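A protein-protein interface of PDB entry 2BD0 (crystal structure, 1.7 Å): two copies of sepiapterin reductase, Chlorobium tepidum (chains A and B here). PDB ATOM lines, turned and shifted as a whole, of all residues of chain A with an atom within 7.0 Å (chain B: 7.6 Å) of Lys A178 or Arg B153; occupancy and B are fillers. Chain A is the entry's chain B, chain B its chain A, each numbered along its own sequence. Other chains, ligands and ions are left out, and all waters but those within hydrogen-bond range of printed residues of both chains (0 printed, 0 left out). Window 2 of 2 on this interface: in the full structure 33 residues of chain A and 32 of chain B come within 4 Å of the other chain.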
ATOM      1  N   GLU A 133       1.788  25.673  18.317  1.00  0.00           N
ATOM      2  CA  GLU A 133       0.783  25.303  17.328  1.00  0.00           C
ATOM      3  C   GLU A 133      -0.379  24.592  18.020  1.00  0.00           C
ATOM      4  O   GLU A 133      -1.544  24.832  17.699  1.00  0.00           O
ATOM      5  CB  GLU A 133       1.397  24.390  16.264  1.00  0.00           C
ATOM      6  CG  GLU A 133       0.586  24.312  14.983  1.00  0.00           C
ATOM      7  CD  GLU A 133       1.281  23.505  13.903  1.00  0.00           C
ATOM      8  OE1 GLU A 133       0.915  23.655  12.718  1.00  0.00           O
ATOM      9  OE2 GLU A 133       2.190  22.715  14.238  1.00  0.00           O
ATOM     10  N   HIS A 136      -2.254  27.105  20.077  1.00  0.00           N
ATOM     11  CA  HIS A 136      -2.960  28.076  19.248  1.00  0.00           C
ATOM     12  C   HIS A 136      -2.656  29.457  19.829  1.00  0.00           C
ATOM     13  O   HIS A 136      -3.511  30.342  19.866  1.00  0.00           O
ATOM     14  CB  HIS A 136      -4.470  27.821  19.250  1.00  0.00           C
ATOM     15  CG  HIS A 136      -5.195  28.495  18.125  1.00  0.00           C
ATOM     16  ND1 HIS A 136      -5.028  28.124  16.807  1.00  0.00           N
ATOM     17  CD2 HIS A 136      -6.068  29.530  18.117  1.00  0.00           C
ATOM     18  CE1 HIS A 136      -5.766  28.904  16.036  1.00  0.00           C
ATOM     19  NE2 HIS A 136      -6.407  29.766  16.805  1.00  0.00           N
ATOM     20  N   THR A 171       9.246  31.459   6.335  1.00  0.00           N
ATOM     21  CA  THR A 171       8.516  30.203   6.223  1.00  0.00           C
ATOM     22  C   THR A 171       7.645  30.044   7.470  1.00  0.00           C
ATOM     23  O   THR A 171       6.506  29.579   7.383  1.00  0.00           O
ATOM     24  CB  THR A 171       9.468  28.993   6.102  1.00  0.00           C
ATOM     25  OG1 THR A 171      10.347  29.179   4.982  1.00  0.00           O
ATOM     26  CG2 THR A 171       8.662  27.706   5.889  1.00  0.00           C
ATOM     27  N   MET A 172       8.169  30.448   8.625  1.00  0.00           N
ATOM     28  CA  MET A 172       7.404  30.341   9.870  1.00  0.00           C
ATOM     29  C   MET A 172       6.135  31.189   9.838  1.00  0.00           C
ATOM     30  O   MET A 172       5.141  30.840  10.470  1.00  0.00           O
ATOM     31  CB  MET A 172       8.253  30.757  11.080  1.00  0.00           C
ATOM     32  CG  MET A 172       9.430  29.837  11.388  1.00  0.00           C
ATOM     33  SD  MET A 172       8.970  28.099  11.593  1.00  0.00           S
ATOM     34  CE  MET A 172       7.845  28.206  13.000  1.00  0.00           C
ATOM     35  N   ARG A 173       6.158  32.305   9.113  1.00  0.00           N
ATOM     36  CA  ARG A 173       4.969  33.152   9.044  1.00  0.00           C
ATOM     37  C   ARG A 173       3.824  32.376   8.405  1.00  0.00           C
ATOM     38  O   ARG A 173       2.668  32.549   8.780  1.00  0.00           O
ATOM     39  CB  ARG A 173       5.233  34.421   8.219  1.00  0.00           C
ATOM     40  CG  ARG A 173       6.264  35.359   8.813  1.00  0.00           C
ATOM     41  CD  ARG A 173       6.344  36.670   8.022  1.00  0.00           C
ATOM     42  NE  ARG A 173       7.470  37.492   8.467  1.00  0.00           N
ATOM     43  CZ  ARG A 173       7.537  38.107   9.646  1.00  0.00           C
ATOM     44  NH1 ARG A 173       6.533  38.006  10.508  1.00  0.00           N
ATOM     45  NH2 ARG A 173       8.617  38.810   9.967  1.00  0.00           N
ATOM     46  N   LEU A 174       4.153  31.524   7.440  1.00  0.00           N
ATOM     47  CA  LEU A 174       3.142  30.736   6.739  1.00  0.00           C
ATOM     48  C   LEU A 174       2.415  29.801   7.695  1.00  0.00           C
ATOM     49  O   LEU A 174       1.202  29.599   7.581  1.00  0.00           O
ATOM     50  CB  LEU A 174       3.786  29.917   5.624  1.00  0.00           C
ATOM     51  CG  LEU A 174       4.576  30.680   4.559  1.00  0.00           C
ATOM     52  CD1 LEU A 174       5.082  29.684   3.519  1.00  0.00           C
ATOM     53  CD2 LEU A 174       3.698  31.741   3.901  1.00  0.00           C
ATOM     54  N   TYR A 175       3.164  29.227   8.629  1.00  0.00           N
ATOM     55  CA  TYR A 175       2.601  28.316   9.617  1.00  0.00           C
ATOM     56  C   TYR A 175       1.905  29.067  10.748  1.00  0.00           C
ATOM     57  O   TYR A 175       0.805  28.707  11.163  1.00  0.00           O
ATOM     58  CB  TYR A 175       3.706  27.445  10.214  1.00  0.00           C
ATOM     59  CG  TYR A 175       4.158  26.320   9.318  1.00  0.00           C
ATOM     60  CD1 TYR A 175       3.500  25.090   9.327  1.00  0.00           C
ATOM     61  CD2 TYR A 175       5.241  26.482   8.457  1.00  0.00           C
ATOM     62  CE1 TYR A 175       3.912  24.048   8.502  1.00  0.00           C
ATOM     63  CE2 TYR A 175       5.661  25.447   7.623  1.00  0.00           C
ATOM     64  CZ  TYR A 175       4.992  24.234   7.654  1.00  0.00           C
ATOM     65  OH  TYR A 175       5.399  23.209   6.835  1.00  0.00           O
ATOM     66  N   ALA A 176       2.565  30.112  11.240  1.00  0.00           N
ATOM     67  CA  ALA A 176       2.056  30.907  12.352  1.00  0.00           C
ATOM     68  C   ALA A 176       0.702  31.569  12.135  1.00  0.00           C
ATOM     69  O   ALA A 176      -0.133  31.584  13.038  1.00  0.00           O
ATOM     70  CB  ALA A 176       3.085  31.966  12.741  1.00  0.00           C
ATOM     71  N   ARG A 177       0.481  32.118  10.947  1.00  0.00           N
ATOM     72  CA  ARG A 177      -0.778  32.797  10.670  1.00  0.00           C
ATOM     73  C   ARG A 177      -2.001  31.894  10.749  1.00  0.00           C
ATOM     74  O   ARG A 177      -3.121  32.379  10.878  1.00  0.00           O
ATOM     75  CB  ARG A 177      -0.713  33.480   9.302  1.00  0.00           C
ATOM     76  CG  ARG A 177       0.190  34.704   9.294  1.00  0.00           C
ATOM     77  CD  ARG A 177       0.502  35.160   7.885  1.00  0.00           C
ATOM     78  NE  ARG A 177       1.318  36.372   7.873  1.00  0.00           N
ATOM     79  CZ  ARG A 177       2.143  36.699   6.882  1.00  0.00           C
ATOM     80  NH1 ARG A 177       2.260  35.897   5.829  1.00  0.00           N
ATOM     81  NH2 ARG A 177       2.842  37.825   6.936  1.00  0.00           N
ATOM     82  N   LYS A 178      -1.791  30.585  10.687  1.00  0.00           N
ATOM     83  CA  LYS A 178      -2.909  29.653  10.745  1.00  0.00           C
ATOM     84  C   LYS A 178      -3.179  29.097  12.137  1.00  0.00           C
ATOM     85  O   LYS A 178      -4.125  28.331  12.328  1.00  0.00           O
ATOM     86  CB  LYS A 178      -2.694  28.506   9.754  1.00  0.00           C
ATOM     87  CG  LYS A 178      -2.785  28.959   8.301  1.00  0.00           C
ATOM     88  CD  LYS A 178      -2.773  27.795   7.332  1.00  0.00           C
ATOM     89  CE  LYS A 178      -2.984  28.287   5.905  1.00  0.00           C
ATOM     90  NZ  LYS A 178      -4.261  29.045   5.759  1.00  0.00           N
ATOM     91  N   CYS A 179      -2.358  29.475  13.112  1.00  0.00           N
ATOM     92  CA  CYS A 179      -2.564  28.988  14.472  1.00  0.00           C
ATOM     93  C   CYS A 179      -2.406  30.052  15.551  1.00  0.00           C
ATOM     94  O   CYS A 179      -2.016  29.751  16.679  1.00  0.00           O
ATOM     95  CB  CYS A 179      -1.648  27.796  14.765  1.00  0.00           C
ATOM     96  SG  CYS A 179       0.110  28.124  14.639  1.00  0.00           S
ATOM     97  N   ASN A 180      -2.695  31.301  15.194  1.00  0.00           N
ATOM     98  CA  ASN A 180      -2.645  32.402  16.149  1.00  0.00           C
ATOM     99  C   ASN A 180      -1.280  32.614  16.803  1.00  0.00           C
ATOM    100  O   ASN A 180      -1.196  32.970  17.980  1.00  0.00           O
ATOM    101  CB  ASN A 180      -3.705  32.163  17.231  1.00  0.00           C
ATOM    102  CG  ASN A 180      -3.968  33.387  18.088  1.00  0.00           C
ATOM    103  OD1 ASN A 180      -4.116  33.282  19.305  1.00  0.00           O
ATOM    104  ND2 ASN A 180      -4.048  34.552  17.456  1.00  0.00           N
ATOM    105  N   VAL A 181      -0.211  32.394  16.048  1.00  0.00           N
ATOM    106  CA  VAL A 181       1.129  32.595  16.580  1.00  0.00           C
ATOM    107  C   VAL A 181       1.739  33.825  15.911  1.00  0.00           C
ATOM    108  O   VAL A 181       1.564  34.035  14.712  1.00  0.00           O
ATOM    109  CB  VAL A 181       2.021  31.354  16.333  1.00  0.00           C
ATOM    110  CG1 VAL A 181       3.465  31.667  16.673  1.00  0.00           C
ATOM    111  CG2 VAL A 181       1.536  30.190  17.198  1.00  0.00           C
ATOM    112  N   PHE B  99      12.411  18.439   0.947  1.00  0.00           N
ATOM    113  CA  PHE B  99      11.172  19.100   1.326  1.00  0.00           C
ATOM    114  C   PHE B  99      10.295  18.284   2.252  1.00  0.00           C
ATOM    115  O   PHE B  99      10.420  17.064   2.330  1.00  0.00           O
ATOM    116  CB  PHE B  99      10.381  19.461   0.070  1.00  0.00           C
ATOM    117  CG  PHE B  99      11.186  20.210  -0.949  1.00  0.00           C
ATOM    118  CD1 PHE B  99      12.034  19.531  -1.821  1.00  0.00           C
ATOM    119  CD2 PHE B  99      11.136  21.600  -1.004  1.00  0.00           C
ATOM    120  CE1 PHE B  99      12.826  20.225  -2.732  1.00  0.00           C
ATOM    121  CE2 PHE B  99      11.924  22.307  -1.911  1.00  0.00           C
ATOM    122  CZ  PHE B  99      12.771  21.620  -2.777  1.00  0.00           C
ATOM    123  N   GLY B 100       9.402  18.975   2.949  1.00  0.00           N
ATOM    124  CA  GLY B 100       8.496  18.311   3.864  1.00  0.00           C
ATOM    125  C   GLY B 100       7.935  19.279   4.880  1.00  0.00           C
ATOM    126  O   GLY B 100       8.439  20.396   5.028  1.00  0.00           O
ATOM    127  N   ALA B 101       6.882  18.863   5.571  1.00  0.00           N
ATOM    128  CA  ALA B 101       6.267  19.704   6.588  1.00  0.00           C
ATOM    129  C   ALA B 101       7.332  20.045   7.621  1.00  0.00           C
ATOM    130  O   ALA B 101       8.245  19.263   7.860  1.00  0.00           O
ATOM    131  CB  ALA B 101       5.110  18.969   7.244  1.00  0.00           C
ATOM    132  N   LEU B 102       7.213  21.221   8.226  1.00  0.00           N
ATOM    133  CA  LEU B 102       8.169  21.676   9.227  1.00  0.00           C
ATOM    134  C   LEU B 102       8.547  20.609  10.253  1.00  0.00           C
ATOM    135  O   LEU B 102       9.727  20.367  10.507  1.00  0.00           O
ATOM    136  CB  LEU B 102       7.603  22.890   9.967  1.00  0.00           C
ATOM    137  CG  LEU B 102       8.430  23.430  11.140  1.00  0.00           C
ATOM    138  CD1 LEU B 102       9.769  23.971  10.639  1.00  0.00           C
ATOM    139  CD2 LEU B 102       7.645  24.527  11.841  1.00  0.00           C
ATOM    140  N   SER B 103       7.536  19.976  10.835  1.00  0.00           N
ATOM    141  CA  SER B 103       7.737  18.962  11.863  1.00  0.00           C
ATOM    142  C   SER B 103       8.381  17.658  11.400  1.00  0.00           C
ATOM    143  O   SER B 103       8.890  16.897  12.225  1.00  0.00           O
ATOM    144  CB  SER B 103       6.398  18.642  12.529  1.00  0.00           C
ATOM    145  OG  SER B 103       5.501  18.070  11.592  1.00  0.00           O
ATOM    146  N   LEU B 105      10.908  17.453   8.971  1.00  0.00           N
ATOM    147  CA  LEU B 105      12.284  17.624   8.519  1.00  0.00           C
ATOM    148  C   LEU B 105      13.293  17.181   9.574  1.00  0.00           C
ATOM    149  O   LEU B 105      13.111  17.425  10.768  1.00  0.00           O
ATOM    150  CB  LEU B 105      12.517  19.080   8.115  1.00  0.00           C
ATOM    151  CG  LEU B 105      11.699  19.471   6.879  1.00  0.00           C
ATOM    152  CD1 LEU B 105      11.762  20.972   6.667  1.00  0.00           C
ATOM    153  CD2 LEU B 105      12.229  18.725   5.654  1.00  0.00           C
ATOM    154  N   ALA B 151       9.033  32.362   0.625  1.00  0.00           N
ATOM    155  CA  ALA B 151       8.942  31.119   1.386  1.00  0.00           C
ATOM    156  C   ALA B 151       7.804  30.232   0.892  1.00  0.00           C
ATOM    157  O   ALA B 151       6.829  30.711   0.308  1.00  0.00           O
ATOM    158  CB  ALA B 151       8.743  31.429   2.870  1.00  0.00           C
ATOM    159  N   PHE B 152       7.952  28.930   1.123  1.00  0.00           N
ATOM    160  CA  PHE B 152       6.946  27.936   0.762  1.00  0.00           C
ATOM    161  C   PHE B 152       6.835  26.984   1.954  1.00  0.00           C
ATOM    162  O   PHE B 152       7.839  26.656   2.588  1.00  0.00           O
ATOM    163  CB  PHE B 152       7.349  27.168  -0.501  1.00  0.00           C
ATOM    164  CG  PHE B 152       7.499  28.039  -1.717  1.00  0.00           C
ATOM    165  CD1 PHE B 152       8.701  28.687  -1.979  1.00  0.00           C
ATOM    166  CD2 PHE B 152       6.436  28.220  -2.593  1.00  0.00           C
ATOM    167  CE1 PHE B 152       8.841  29.506  -3.099  1.00  0.00           C
ATOM    168  CE2 PHE B 152       6.564  29.039  -3.717  1.00  0.00           C
ATOM    169  CZ  PHE B 152       7.767  29.681  -3.970  1.00  0.00           C
ATOM    170  N   ARG B 153       5.616  26.544   2.252  1.00  0.00           N
ATOM    171  CA  ARG B 153       5.359  25.673   3.399  1.00  0.00           C
ATOM    172  C   ARG B 153       6.286  24.483   3.634  1.00  0.00           C
ATOM    173  O   ARG B 153       6.764  24.280   4.751  1.00  0.00           O
ATOM    174  CB  ARG B 153       3.905  25.196   3.363  1.00  0.00           C
ATOM    175  CG  ARG B 153       2.929  26.312   3.687  1.00  0.00           C
ATOM    176  CD  ARG B 153       1.481  25.864   3.637  1.00  0.00           C
ATOM    177  NE  ARG B 153       0.575  26.964   3.970  1.00  0.00           N
ATOM    178  CZ  ARG B 153       0.512  28.112   3.301  1.00  0.00           C
ATOM    179  NH1 ARG B 153       1.301  28.322   2.256  1.00  0.00           N
ATOM    180  NH2 ARG B 153      -0.340  29.057   3.679  1.00  0.00           N
ATOM    181  N   HIS B 154       6.542  23.690   2.604  1.00  0.00           N
ATOM    182  CA  HIS B 154       7.418  22.538   2.781  1.00  0.00           C
ATOM    183  C   HIS B 154       8.875  22.837   2.447  1.00  0.00           C
ATOM    184  O   HIS B 154       9.680  21.920   2.285  1.00  0.00           O
ATOM    185  CB  HIS B 154       6.914  21.362   1.942  1.00  0.00           C
ATOM    186  CG  HIS B 154       5.648  20.754   2.461  1.00  0.00           C
ATOM    187  ND1 HIS B 154       5.153  19.556   1.996  1.00  0.00           N
ATOM    188  CD2 HIS B 154       4.780  21.176   3.411  1.00  0.00           C
ATOM    189  CE1 HIS B 154       4.035  19.264   2.637  1.00  0.00           C
ATOM    190  NE2 HIS B 154       3.787  20.231   3.502  1.00  0.00           N
ATOM    191  N   SER B 155       9.219  24.121   2.369  1.00  0.00           N
ATOM    192  CA  SER B 155      10.583  24.519   2.033  1.00  0.00           C
ATOM    193  C   SER B 155      11.341  25.268   3.127  1.00  0.00           C
ATOM    194  O   SER B 155      12.196  26.093   2.818  1.00  0.00           O
ATOM    195  CB  SER B 155      10.573  25.386   0.767  1.00  0.00           C
ATOM    196  OG  SER B 155       9.954  24.713  -0.315  1.00  0.00           O
ATOM    197  N   SER B 156      11.053  24.990   4.396  1.00  0.00           N
ATOM    198  CA  SER B 156      11.755  25.690   5.475  1.00  0.00           C
ATOM    199  C   SER B 156      13.275  25.559   5.354  1.00  0.00           C
ATOM    200  O   SER B 156      14.002  26.557   5.415  1.00  0.00           O
ATOM    201  CB  SER B 156      11.292  25.181   6.845  1.00  0.00           C
ATOM    202  OG  SER B 156      11.513  23.794   6.990  1.00  0.00           O
ATOM    203  N   ILE B 157      13.761  24.337   5.178  1.00  0.00           N
ATOM    204  CA  ILE B 157      15.197  24.128   5.050  1.00  0.00           C
ATOM    205  C   ILE B 157      15.704  24.582   3.680  1.00  0.00           C
ATOM    206  O   ILE B 157      16.777  25.176   3.576  1.00  0.00           O
ATOM    207  CB  ILE B 157      15.563  22.645   5.283  1.00  0.00           C
ATOM    208  CG1 ILE B 157      15.312  22.288   6.750  1.00  0.00           C
ATOM    209  CG2 ILE B 157      17.020  22.389   4.919  1.00  0.00           C
ATOM    210  CD1 ILE B 157      15.547  20.820   7.082  1.00  0.00           C
ATOM    211  N   CYS B 159      14.493  26.933   1.773  1.00  0.00           N
ATOM    212  CA  CYS B 159      14.523  28.393   1.777  1.00  0.00           C
ATOM    213  C   CYS B 159      15.683  28.937   2.607  1.00  0.00           C
ATOM    214  O   CYS B 159      16.303  29.929   2.226  1.00  0.00           O
ATOM    215  CB  CYS B 159      13.188  28.958   2.279  1.00  0.00           C
ATOM    216  SG  CYS B 159      11.843  28.768   1.083  1.00  0.00           S
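No position is printed for both chains.
The backbone carbonyl oxygen (O) of Ser B155 sits close to the side-chain sulfur (SG) of Cys B159, at 3.2 Å.
The backbone carbonyl oxygen (O) of Tyr A175 sits at hydrogen-bond distance from the side-chain sulfur (SG) of Cys A179.
The backbone NH (N) of Leu B102 sits at hydrogen-bond distance from the side-chain hydroxyl (OH) of Tyr A175.
The backbone carbonyl oxygen of Arg B153 sits at hydrogen-bond distance from the side-chain hydroxyl of Tyr A175, at 2.7 Å.
Printed residues of chain B that touch a printed residue of chain A: Ala B101, Leu B102, Ala B151, Phe B152, Arg B153, Ser B156 and Cys B159.
Hydrophobic or aromatic side chains of chain B within 4 Å of the printed part of chain A: Leu B102 and Ala B151.
Among the printed residues, 12 pairs touch across the chains.
Of the printed residues of chain A, Arg B153 touches Leu A174, Tyr A175 and Lys A178.
Of the printed residues of chain A, Leu B102 touches Met A172 (3.8 Å) and Tyr A175 (3.0 Å).
Printed residues of chain B within 4 Å of Leu A174: Ala B151, Phe B152 and Arg B153.
Of the printed residues of chain A, Phe B152 touches Thr A171 (3.6 Å) and Leu A174 (3.6 Å).
Phe B99 touches none of the printed residues of chain A.
Arg A177 touches none of the printed residues of chain B.
The nearest printed residue of chain B that does not touch Lys A178 is Phe B152 (10.7 Å).
Among the printed residues, merely in contact across the chains: Thr A171 with Ala B151 (3.5 Å), Thr A171 with Phe B152 (3.6 Å), Thr A171 with Ser B156 (3.7 Å), Thr A171 with Cys B159 (3.9 Å), Met A172 with Leu B102 (3.8 Å), Leu A174 with Ala B151 (3.8 Å), Leu A174 with Phe B152 (3.6 Å), Leu A174 with Arg B153 (3.4 Å), Tyr A175 with Ala B101 (3.6 Å) and Lys A178 with Arg B153 (3.5 Å).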
